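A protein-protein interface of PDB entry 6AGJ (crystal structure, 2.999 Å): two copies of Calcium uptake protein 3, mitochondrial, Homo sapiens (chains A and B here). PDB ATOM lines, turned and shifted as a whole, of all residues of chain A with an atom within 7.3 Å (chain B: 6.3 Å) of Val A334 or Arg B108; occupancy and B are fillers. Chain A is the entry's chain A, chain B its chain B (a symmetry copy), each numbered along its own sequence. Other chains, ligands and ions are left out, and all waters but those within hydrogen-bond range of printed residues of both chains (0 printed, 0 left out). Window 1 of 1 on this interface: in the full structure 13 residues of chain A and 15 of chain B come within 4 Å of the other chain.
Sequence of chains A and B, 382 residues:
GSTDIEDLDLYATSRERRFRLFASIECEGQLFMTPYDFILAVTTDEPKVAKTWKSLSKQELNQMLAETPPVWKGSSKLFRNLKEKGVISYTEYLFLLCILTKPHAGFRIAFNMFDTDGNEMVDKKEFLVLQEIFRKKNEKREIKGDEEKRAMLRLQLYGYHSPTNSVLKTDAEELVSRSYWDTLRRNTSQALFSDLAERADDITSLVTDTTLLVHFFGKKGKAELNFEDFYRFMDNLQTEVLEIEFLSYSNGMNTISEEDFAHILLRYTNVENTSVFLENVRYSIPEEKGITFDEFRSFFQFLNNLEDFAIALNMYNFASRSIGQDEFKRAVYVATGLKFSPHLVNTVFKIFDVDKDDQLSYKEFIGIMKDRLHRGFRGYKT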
ATOM      1  N   ASP A 308      32.197 -13.745  -7.065  1.00  0.00           N
ATOM      2  CA  ASP A 308      31.046 -14.571  -6.739  1.00  0.00           C
ATOM      3  C   ASP A 308      31.210 -16.001  -7.234  1.00  0.00           C
ATOM      4  O   ASP A 308      30.684 -16.929  -6.606  1.00  0.00           O
ATOM      5  CB  ASP A 308      29.784 -13.925  -7.294  1.00  0.00           C
ATOM      6  CG  ASP A 308      29.695 -12.443  -6.953  1.00  0.00           C
ATOM      7  OD1 ASP A 308      29.400 -12.105  -5.771  1.00  0.00           O
ATOM      8  OD2 ASP A 308      29.982 -11.621  -7.869  1.00  0.00           O
ATOM      9  N   PHE A 309      31.945 -16.213  -8.334  1.00  0.00           N
ATOM     10  CA  PHE A 309      32.233 -17.594  -8.735  1.00  0.00           C
ATOM     11  C   PHE A 309      33.001 -18.333  -7.648  1.00  0.00           C
ATOM     12  O   PHE A 309      32.681 -19.483  -7.314  1.00  0.00           O
ATOM     13  CB  PHE A 309      33.021 -17.612 -10.038  1.00  0.00           C
ATOM     14  CG  PHE A 309      33.394 -18.996 -10.526  1.00  0.00           C
ATOM     15  CD1 PHE A 309      32.432 -19.863 -11.002  1.00  0.00           C
ATOM     16  CD2 PHE A 309      34.728 -19.398 -10.571  1.00  0.00           C
ATOM     17  CE1 PHE A 309      32.793 -21.122 -11.485  1.00  0.00           C
ATOM     18  CE2 PHE A 309      35.091 -20.649 -11.046  1.00  0.00           C
ATOM     19  CZ  PHE A 309      34.123 -21.511 -11.506  1.00  0.00           C
ATOM     20  N   ALA A 312      30.682 -19.066  -4.652  1.00  0.00           N
ATOM     21  CA  ALA A 312      29.829 -20.192  -4.957  1.00  0.00           C
ATOM     22  C   ALA A 312      30.585 -21.503  -4.878  1.00  0.00           C
ATOM     23  O   ALA A 312      30.034 -22.512  -4.427  1.00  0.00           O
ATOM     24  CB  ALA A 312      29.211 -19.964  -6.330  1.00  0.00           C
ATOM     25  N   PHE A 328      31.744 -27.567 -13.581  1.00  0.00           N
ATOM     26  CA  PHE A 328      32.280 -26.219 -13.810  1.00  0.00           C
ATOM     27  C   PHE A 328      31.267 -25.364 -14.557  1.00  0.00           C
ATOM     28  O   PHE A 328      31.070 -24.181 -14.243  1.00  0.00           O
ATOM     29  CB  PHE A 328      33.597 -26.313 -14.610  1.00  0.00           C
ATOM     30  CG  PHE A 328      34.249 -24.971 -14.966  1.00  0.00           C
ATOM     31  CD1 PHE A 328      33.742 -24.143 -15.971  1.00  0.00           C
ATOM     32  CD2 PHE A 328      35.436 -24.590 -14.352  1.00  0.00           C
ATOM     33  CE1 PHE A 328      34.372 -22.929 -16.290  1.00  0.00           C
ATOM     34  CE2 PHE A 328      36.070 -23.374 -14.678  1.00  0.00           C
ATOM     35  CZ  PHE A 328      35.534 -22.553 -15.639  1.00  0.00           C
ATOM     36  N   LYS A 329      30.618 -25.961 -15.551  1.00  0.00           N
ATOM     37  CA  LYS A 329      29.584 -25.272 -16.307  1.00  0.00           C
ATOM     38  C   LYS A 329      28.455 -24.812 -15.387  1.00  0.00           C
ATOM     39  O   LYS A 329      28.087 -23.623 -15.375  1.00  0.00           O
ATOM     40  CB  LYS A 329      29.099 -26.198 -17.431  1.00  0.00           C
ATOM     41  CG  LYS A 329      27.809 -25.808 -18.120  1.00  0.00           C
ATOM     42  CD  LYS A 329      27.766 -26.419 -19.523  1.00  0.00           C
ATOM     43  CE  LYS A 329      26.843 -25.638 -20.449  1.00  0.00           C
ATOM     44  NZ  LYS A 329      25.879 -24.824 -19.651  1.00  0.00           N
ATOM     45  N   ARG A 330      27.906 -25.743 -14.595  1.00  0.00           N
ATOM     46  CA  ARG A 330      26.858 -25.394 -13.636  1.00  0.00           C
ATOM     47  C   ARG A 330      27.304 -24.255 -12.722  1.00  0.00           C
ATOM     48  O   ARG A 330      26.586 -23.262 -12.556  1.00  0.00           O
ATOM     49  CB  ARG A 330      26.454 -26.628 -12.824  1.00  0.00           C
ATOM     50  CG  ARG A 330      24.929 -26.965 -12.822  1.00  0.00           C
ATOM     51  CD  ARG A 330      24.655 -28.416 -12.344  1.00  0.00           C
ATOM     52  NE  ARG A 330      25.543 -28.763 -11.233  1.00  0.00           N
ATOM     53  CZ  ARG A 330      26.450 -29.739 -11.249  1.00  0.00           C
ATOM     54  NH1 ARG A 330      26.585 -30.506 -12.327  1.00  0.00           N
ATOM     55  NH2 ARG A 330      27.221 -29.947 -10.179  1.00  0.00           N
ATOM     56  N   ALA A 331      28.499 -24.380 -12.131  1.00  0.00           N
ATOM     57  CA  ALA A 331      29.046 -23.347 -11.253  1.00  0.00           C
ATOM     58  C   ALA A 331      29.044 -21.970 -11.916  1.00  0.00           C
ATOM     59  O   ALA A 331      28.643 -20.965 -11.310  1.00  0.00           O
ATOM     60  CB  ALA A 331      30.454 -23.745 -10.833  1.00  0.00           C
ATOM     61  N   VAL A 332      29.521 -21.897 -13.161  1.00  0.00           N
ATOM     62  CA  VAL A 332      29.493 -20.628 -13.884  1.00  0.00           C
ATOM     63  C   VAL A 332      28.076 -20.090 -13.941  1.00  0.00           C
ATOM     64  O   VAL A 332      27.807 -18.950 -13.538  1.00  0.00           O
ATOM     65  CB  VAL A 332      30.078 -20.795 -15.297  1.00  0.00           C
ATOM     66  CG1 VAL A 332      29.916 -19.513 -16.090  1.00  0.00           C
ATOM     67  CG2 VAL A 332      31.518 -21.190 -15.212  1.00  0.00           C
ATOM     68  N   TYR A 333      27.139 -20.919 -14.411  1.00  0.00           N
ATOM     69  CA  TYR A 333      25.770 -20.444 -14.569  1.00  0.00           C
ATOM     70  C   TYR A 333      25.223 -19.865 -13.277  1.00  0.00           C
ATOM     71  O   TYR A 333      24.813 -18.701 -13.218  1.00  0.00           O
ATOM     72  CB  TYR A 333      24.844 -21.571 -15.016  1.00  0.00           C
ATOM     73  CG  TYR A 333      23.438 -21.036 -15.177  1.00  0.00           C
ATOM     74  CD1 TYR A 333      23.183 -19.953 -16.021  1.00  0.00           C
ATOM     75  CD2 TYR A 333      22.398 -21.507 -14.380  1.00  0.00           C
ATOM     76  CE1 TYR A 333      21.913 -19.434 -16.149  1.00  0.00           C
ATOM     77  CE2 TYR A 333      21.126 -20.989 -14.492  1.00  0.00           C
ATOM     78  CZ  TYR A 333      20.883 -19.952 -15.380  1.00  0.00           C
ATOM     79  OH  TYR A 333      19.609 -19.426 -15.500  1.00  0.00           O
ATOM     80  N   VAL A 334      25.199 -20.696 -12.234  1.00  0.00           N
ATOM     81  CA  VAL A 334      24.634 -20.306 -10.949  1.00  0.00           C
ATOM     82  C   VAL A 334      25.265 -19.023 -10.436  1.00  0.00           C
ATOM     83  O   VAL A 334      24.567 -18.068 -10.075  1.00  0.00           O
ATOM     84  CB  VAL A 334      24.798 -21.452  -9.944  1.00  0.00           C
ATOM     85  CG1 VAL A 334      24.475 -20.971  -8.549  1.00  0.00           C
ATOM     86  CG2 VAL A 334      23.886 -22.593 -10.370  1.00  0.00           C
ATOM     87  N   ALA A 335      26.597 -18.978 -10.399  1.00  0.00           N
ATOM     88  CA  ALA A 335      27.271 -17.842  -9.782  1.00  0.00           C
ATOM     89  C   ALA A 335      27.283 -16.580 -10.634  1.00  0.00           C
ATOM     90  O   ALA A 335      27.692 -15.534 -10.130  1.00  0.00           O
ATOM     91  CB  ALA A 335      28.715 -18.205  -9.441  1.00  0.00           C
ATOM     92  N   THR A 336      26.896 -16.645 -11.908  1.00  0.00           N
ATOM     93  CA  THR A 336      27.014 -15.476 -12.781  1.00  0.00           C
ATOM     94  C   THR A 336      25.880 -15.302 -13.767  1.00  0.00           C
ATOM     95  O   THR A 336      25.860 -14.282 -14.465  1.00  0.00           O
ATOM     96  CB  THR A 336      28.312 -15.508 -13.599  1.00  0.00           C
ATOM     97  OG1 THR A 336      28.279 -16.635 -14.494  1.00  0.00           O
ATOM     98  CG2 THR A 336      29.570 -15.517 -12.713  1.00  0.00           C
ATOM     99  N   GLY A 337      24.996 -16.281 -13.927  1.00  0.00           N
ATOM    100  CA  GLY A 337      23.948 -16.188 -14.905  1.00  0.00           C
ATOM    101  C   GLY A 337      24.318 -16.602 -16.299  1.00  0.00           C
ATOM    102  O   GLY A 337      23.414 -16.817 -17.111  1.00  0.00           O
ATOM    103  N   LEU A 338      25.608 -16.740 -16.623  1.00  0.00           N
ATOM    104  CA  LEU A 338      25.989 -17.026 -18.001  1.00  0.00           C
ATOM    105  C   LEU A 338      26.033 -18.517 -18.267  1.00  0.00           C
ATOM    106  O   LEU A 338      26.466 -19.307 -17.421  1.00  0.00           O
ATOM    107  CB  LEU A 338      27.343 -16.422 -18.371  1.00  0.00           C
ATOM    108  CG  LEU A 338      27.575 -14.937 -18.116  1.00  0.00           C
ATOM    109  CD1 LEU A 338      28.624 -14.635 -17.025  1.00  0.00           C
ATOM    110  CD2 LEU A 338      27.938 -14.298 -19.438  1.00  0.00           C
ATOM    111  N   HIS B 104      20.212 -15.236   2.504  1.00  0.00           N
ATOM    112  CA  HIS B 104      19.561 -16.293   1.736  1.00  0.00           C
ATOM    113  C   HIS B 104      20.433 -16.786   0.598  1.00  0.00           C
ATOM    114  O   HIS B 104      20.451 -17.994   0.316  1.00  0.00           O
ATOM    115  CB  HIS B 104      18.222 -15.815   1.161  1.00  0.00           C
ATOM    116  CG  HIS B 104      17.655 -16.737   0.120  1.00  0.00           C
ATOM    117  ND1 HIS B 104      17.815 -16.521  -1.233  1.00  0.00           N
ATOM    118  CD2 HIS B 104      16.946 -17.888   0.234  1.00  0.00           C
ATOM    119  CE1 HIS B 104      17.229 -17.496  -1.907  1.00  0.00           C
ATOM    120  NE2 HIS B 104      16.692 -18.337  -1.041  1.00  0.00           N
ATOM    121  N   ALA B 105      21.254 -15.896   0.034  1.00  0.00           N
ATOM    122  CA  ALA B 105      21.930 -16.180  -1.226  1.00  0.00           C
ATOM    123  C   ALA B 105      22.612 -17.541  -1.185  1.00  0.00           C
ATOM    124  O   ALA B 105      22.383 -18.390  -2.057  1.00  0.00           O
ATOM    125  CB  ALA B 105      22.934 -15.072  -1.520  1.00  0.00           C
ATOM    126  N   GLY B 106      23.435 -17.769  -0.154  1.00  0.00           N
ATOM    127  CA  GLY B 106      24.198 -19.001  -0.051  1.00  0.00           C
ATOM    128  C   GLY B 106      23.353 -20.250  -0.142  1.00  0.00           C
ATOM    129  O   GLY B 106      23.822 -21.301  -0.619  1.00  0.00           O
ATOM    130  N   PHE B 107      22.112 -20.177   0.336  1.00  0.00           N
ATOM    131  CA  PHE B 107      21.239 -21.334   0.222  1.00  0.00           C
ATOM    132  C   PHE B 107      20.801 -21.553  -1.225  1.00  0.00           C
ATOM    133  O   PHE B 107      20.875 -22.681  -1.741  1.00  0.00           O
ATOM    134  CB  PHE B 107      20.056 -21.182   1.168  1.00  0.00           C
ATOM    135  CG  PHE B 107      20.378 -21.564   2.567  1.00  0.00           C
ATOM    136  CD1 PHE B 107      20.360 -22.901   2.942  1.00  0.00           C
ATOM    137  CD2 PHE B 107      20.724 -20.603   3.511  1.00  0.00           C
ATOM    138  CE1 PHE B 107      20.666 -23.281   4.251  1.00  0.00           C
ATOM    139  CE2 PHE B 107      21.032 -20.965   4.821  1.00  0.00           C
ATOM    140  CZ  PHE B 107      21.007 -22.312   5.194  1.00  0.00           C
ATOM    141  N   ARG B 108      20.386 -20.479  -1.914  1.00  0.00           N
ATOM    142  CA  ARG B 108      20.102 -20.617  -3.335  1.00  0.00           C
ATOM    143  C   ARG B 108      21.322 -21.187  -4.048  1.00  0.00           C
ATOM    144  O   ARG B 108      21.192 -22.024  -4.955  1.00  0.00           O
ATOM    145  CB  ARG B 108      19.686 -19.287  -3.967  1.00  0.00           C
ATOM    146  CG  ARG B 108      20.768 -18.781  -4.930  1.00  0.00           C
ATOM    147  CD  ARG B 108      20.470 -17.550  -5.773  1.00  0.00           C
ATOM    148  NE  ARG B 108      21.681 -17.272  -6.546  1.00  0.00           N
ATOM    149  CZ  ARG B 108      22.026 -17.909  -7.665  1.00  0.00           C
ATOM    150  NH1 ARG B 108      21.248 -18.871  -8.152  1.00  0.00           N
ATOM    151  NH2 ARG B 108      23.169 -17.610  -8.282  1.00  0.00           N
ATOM    152  N   ILE B 109      22.519 -20.797  -3.605  1.00  0.00           N
ATOM    153  CA  ILE B 109      23.725 -21.285  -4.247  1.00  0.00           C
ATOM    154  C   ILE B 109      23.801 -22.795  -4.128  1.00  0.00           C
ATOM    155  O   ILE B 109      23.791 -23.514  -5.130  1.00  0.00           O
ATOM    156  CB  ILE B 109      24.967 -20.677  -3.592  1.00  0.00           C
ATOM    157  CG1 ILE B 109      25.116 -19.202  -3.919  1.00  0.00           C
ATOM    158  CG2 ILE B 109      26.209 -21.443  -4.061  1.00  0.00           C
ATOM    159  CD1 ILE B 109      25.007 -18.912  -5.389  1.00  0.00           C
ATOM    160  N   ALA B 110      23.841 -23.309  -2.891  1.00  0.00           N
ATOM    161  CA  ALA B 110      24.122 -24.737  -2.756  1.00  0.00           C
ATOM    162  C   ALA B 110      22.955 -25.609  -3.223  1.00  0.00           C
ATOM    163  O   ALA B 110      23.158 -26.758  -3.647  1.00  0.00           O
ATOM    164  CB  ALA B 110      24.533 -25.064  -1.333  1.00  0.00           C
ATOM    165  N   PHE B 111      21.720 -25.126  -3.113  1.00  0.00           N
ATOM    166  CA  PHE B 111      20.629 -25.942  -3.634  1.00  0.00           C
ATOM    167  C   PHE B 111      20.704 -26.007  -5.152  1.00  0.00           C
ATOM    168  O   PHE B 111      20.600 -27.088  -5.746  1.00  0.00           O
ATOM    169  CB  PHE B 111      19.276 -25.426  -3.155  1.00  0.00           C
ATOM    170  CG  PHE B 111      18.810 -26.096  -1.894  1.00  0.00           C
ATOM    171  CD1 PHE B 111      19.537 -25.965  -0.720  1.00  0.00           C
ATOM    172  CD2 PHE B 111      17.690 -26.910  -1.892  1.00  0.00           C
ATOM    173  CE1 PHE B 111      19.118 -26.590   0.454  1.00  0.00           C
ATOM    174  CE2 PHE B 111      17.263 -27.545  -0.718  1.00  0.00           C
ATOM    175  CZ  PHE B 111      17.976 -27.387   0.453  1.00  0.00           C
ATOM    176  N   ASN B 112      20.890 -24.856  -5.803  1.00  0.00           N
ATOM    177  CA  ASN B 112      21.078 -24.881  -7.245  1.00  0.00           C
ATOM    178  C   ASN B 112      22.266 -25.764  -7.630  1.00  0.00           C
ATOM    179  O   ASN B 112      22.208 -26.494  -8.619  1.00  0.00           O
ATOM    180  CB  ASN B 112      21.254 -23.457  -7.747  1.00  0.00           C
ATOM    181  CG  ASN B 112      19.938 -22.781  -8.006  1.00  0.00           C
ATOM    182  OD1 ASN B 112      19.814 -21.570  -7.872  1.00  0.00           O
ATOM    183  ND2 ASN B 112      18.943 -23.561  -8.390  1.00  0.00           N
ATOM    184  N   MET B 113      23.328 -25.715  -6.841  1.00  0.00           N
ATOM    185  CA  MET B 113      24.497 -26.534  -7.112  1.00  0.00           C
ATOM    186  C   MET B 113      24.216 -28.031  -7.027  1.00  0.00           C
ATOM    187  O   MET B 113      24.706 -28.793  -7.851  1.00  0.00           O
ATOM    188  CB  MET B 113      25.657 -26.152  -6.202  1.00  0.00           C
ATOM    189  CG  MET B 113      26.506 -25.004  -6.724  1.00  0.00           C
ATOM    190  SD  MET B 113      27.294 -25.328  -8.306  1.00  0.00           S
ATOM    191  CE  MET B 113      26.051 -24.716  -9.412  1.00  0.00           C
ATOM    192  N   PHE B 227      12.276 -26.527  -4.337  1.00  0.00           N
ATOM    193  CA  PHE B 227      12.945 -25.318  -3.865  1.00  0.00           C
ATOM    194  C   PHE B 227      11.966 -24.341  -3.217  1.00  0.00           C
ATOM    195  O   PHE B 227      12.267 -23.777  -2.158  1.00  0.00           O
ATOM    196  CB  PHE B 227      13.667 -24.617  -5.015  1.00  0.00           C
ATOM    197  CG  PHE B 227      14.969 -25.262  -5.426  1.00  0.00           C
ATOM    198  CD1 PHE B 227      15.317 -26.529  -4.973  1.00  0.00           C
ATOM    199  CD2 PHE B 227      15.856 -24.578  -6.258  1.00  0.00           C
ATOM    200  CE1 PHE B 227      16.507 -27.122  -5.365  1.00  0.00           C
ATOM    201  CE2 PHE B 227      17.035 -25.152  -6.644  1.00  0.00           C
ATOM    202  CZ  PHE B 227      17.368 -26.435  -6.193  1.00  0.00           C
ATOM    203  N   TYR B 231      12.507 -22.826   0.593  1.00  0.00           N
ATOM    204  CA  TYR B 231      12.744 -21.419   0.869  1.00  0.00           C
ATOM    205  C   TYR B 231      11.644 -20.881   1.771  1.00  0.00           C
ATOM    206  O   TYR B 231      11.884 -20.027   2.633  1.00  0.00           O
ATOM    207  CB  TYR B 231      12.806 -20.616  -0.429  1.00  0.00           C
ATOM    208  CG  TYR B 231      13.985 -20.952  -1.317  1.00  0.00           C
ATOM    209  CD1 TYR B 231      15.180 -21.397  -0.778  1.00  0.00           C
ATOM    210  CD2 TYR B 231      13.895 -20.840  -2.707  1.00  0.00           C
ATOM    211  CE1 TYR B 231      16.256 -21.718  -1.596  1.00  0.00           C
ATOM    212  CE2 TYR B 231      14.963 -21.154  -3.522  1.00  0.00           C
ATOM    213  CZ  TYR B 231      16.140 -21.594  -2.964  1.00  0.00           C
ATOM    214  OH  TYR B 231      17.216 -21.913  -3.777  1.00  0.00           O
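NE of Arg A330 is in hydrogen-bond range of O of Met B113, at 3.5 Å. The backbone carbonyl oxygen (O) of Val A334 lies close to the guanidinium group (NH2) of Arg B108 (2.3 Å).
Printed residues of chain B within 4 Å of Ala A312: Ile B109 (3.9 Å). Of the printed residues of chain B, Arg A330 touches Met B113 (3.5 Å). Val A334 touches just these residues of chain B: Arg B108 (2.3 Å), Ile B109 (3.8 Å), Asn B112 (3.8 Å) and Met B113 (3.2 Å). Of chain A, only Val A334 comes within 4 Å of Arg B108. Printed residues of chain A within 4 Å of Ile B109: Ala A312 and Val A334. Printed residues of chain A within 4 Å of Asn B112: Val A334. Printed residues of chain A within 4 Å of Met B113: Arg A330 (3.5 Å), Ala A331 (3.7 Å) and Val A334 (3.2 Å). The nearest residue of chain A that does not touch Arg B108 is Ala A335 (4.3 Å). The nearest printed residue of chain A that does not touch Asn B112 is Arg A330 (4.8 Å).
Among the printed residues, pairs that only touch across the chains: Val A334 with Met B113 (3.2 Å), Ala A331 with Met B113 (3.7 Å), Val A334 with Ile B109 (3.8 Å), Val A334 with Asn B112 (3.8 Å) and Ala A312 with Ile B109 (3.9 Å).
No position is printed for both chains. Of the 7 pairs that touch across the chains among the printed residues, none has its exchanged pair printed and touching as well.
NH1 of Arg B108 lies within hydrogen-bond range of OD1 of Asn B112 (3.1 Å).
Of the 12 printed residues of chain B, 4 touch a printed residue of chain A. Hydrophobic or aromatic side chains of chain B that line the printed part of chain A: Ile B109 and Met B113. Among the printed residues, 7 pairs touch across the chains.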
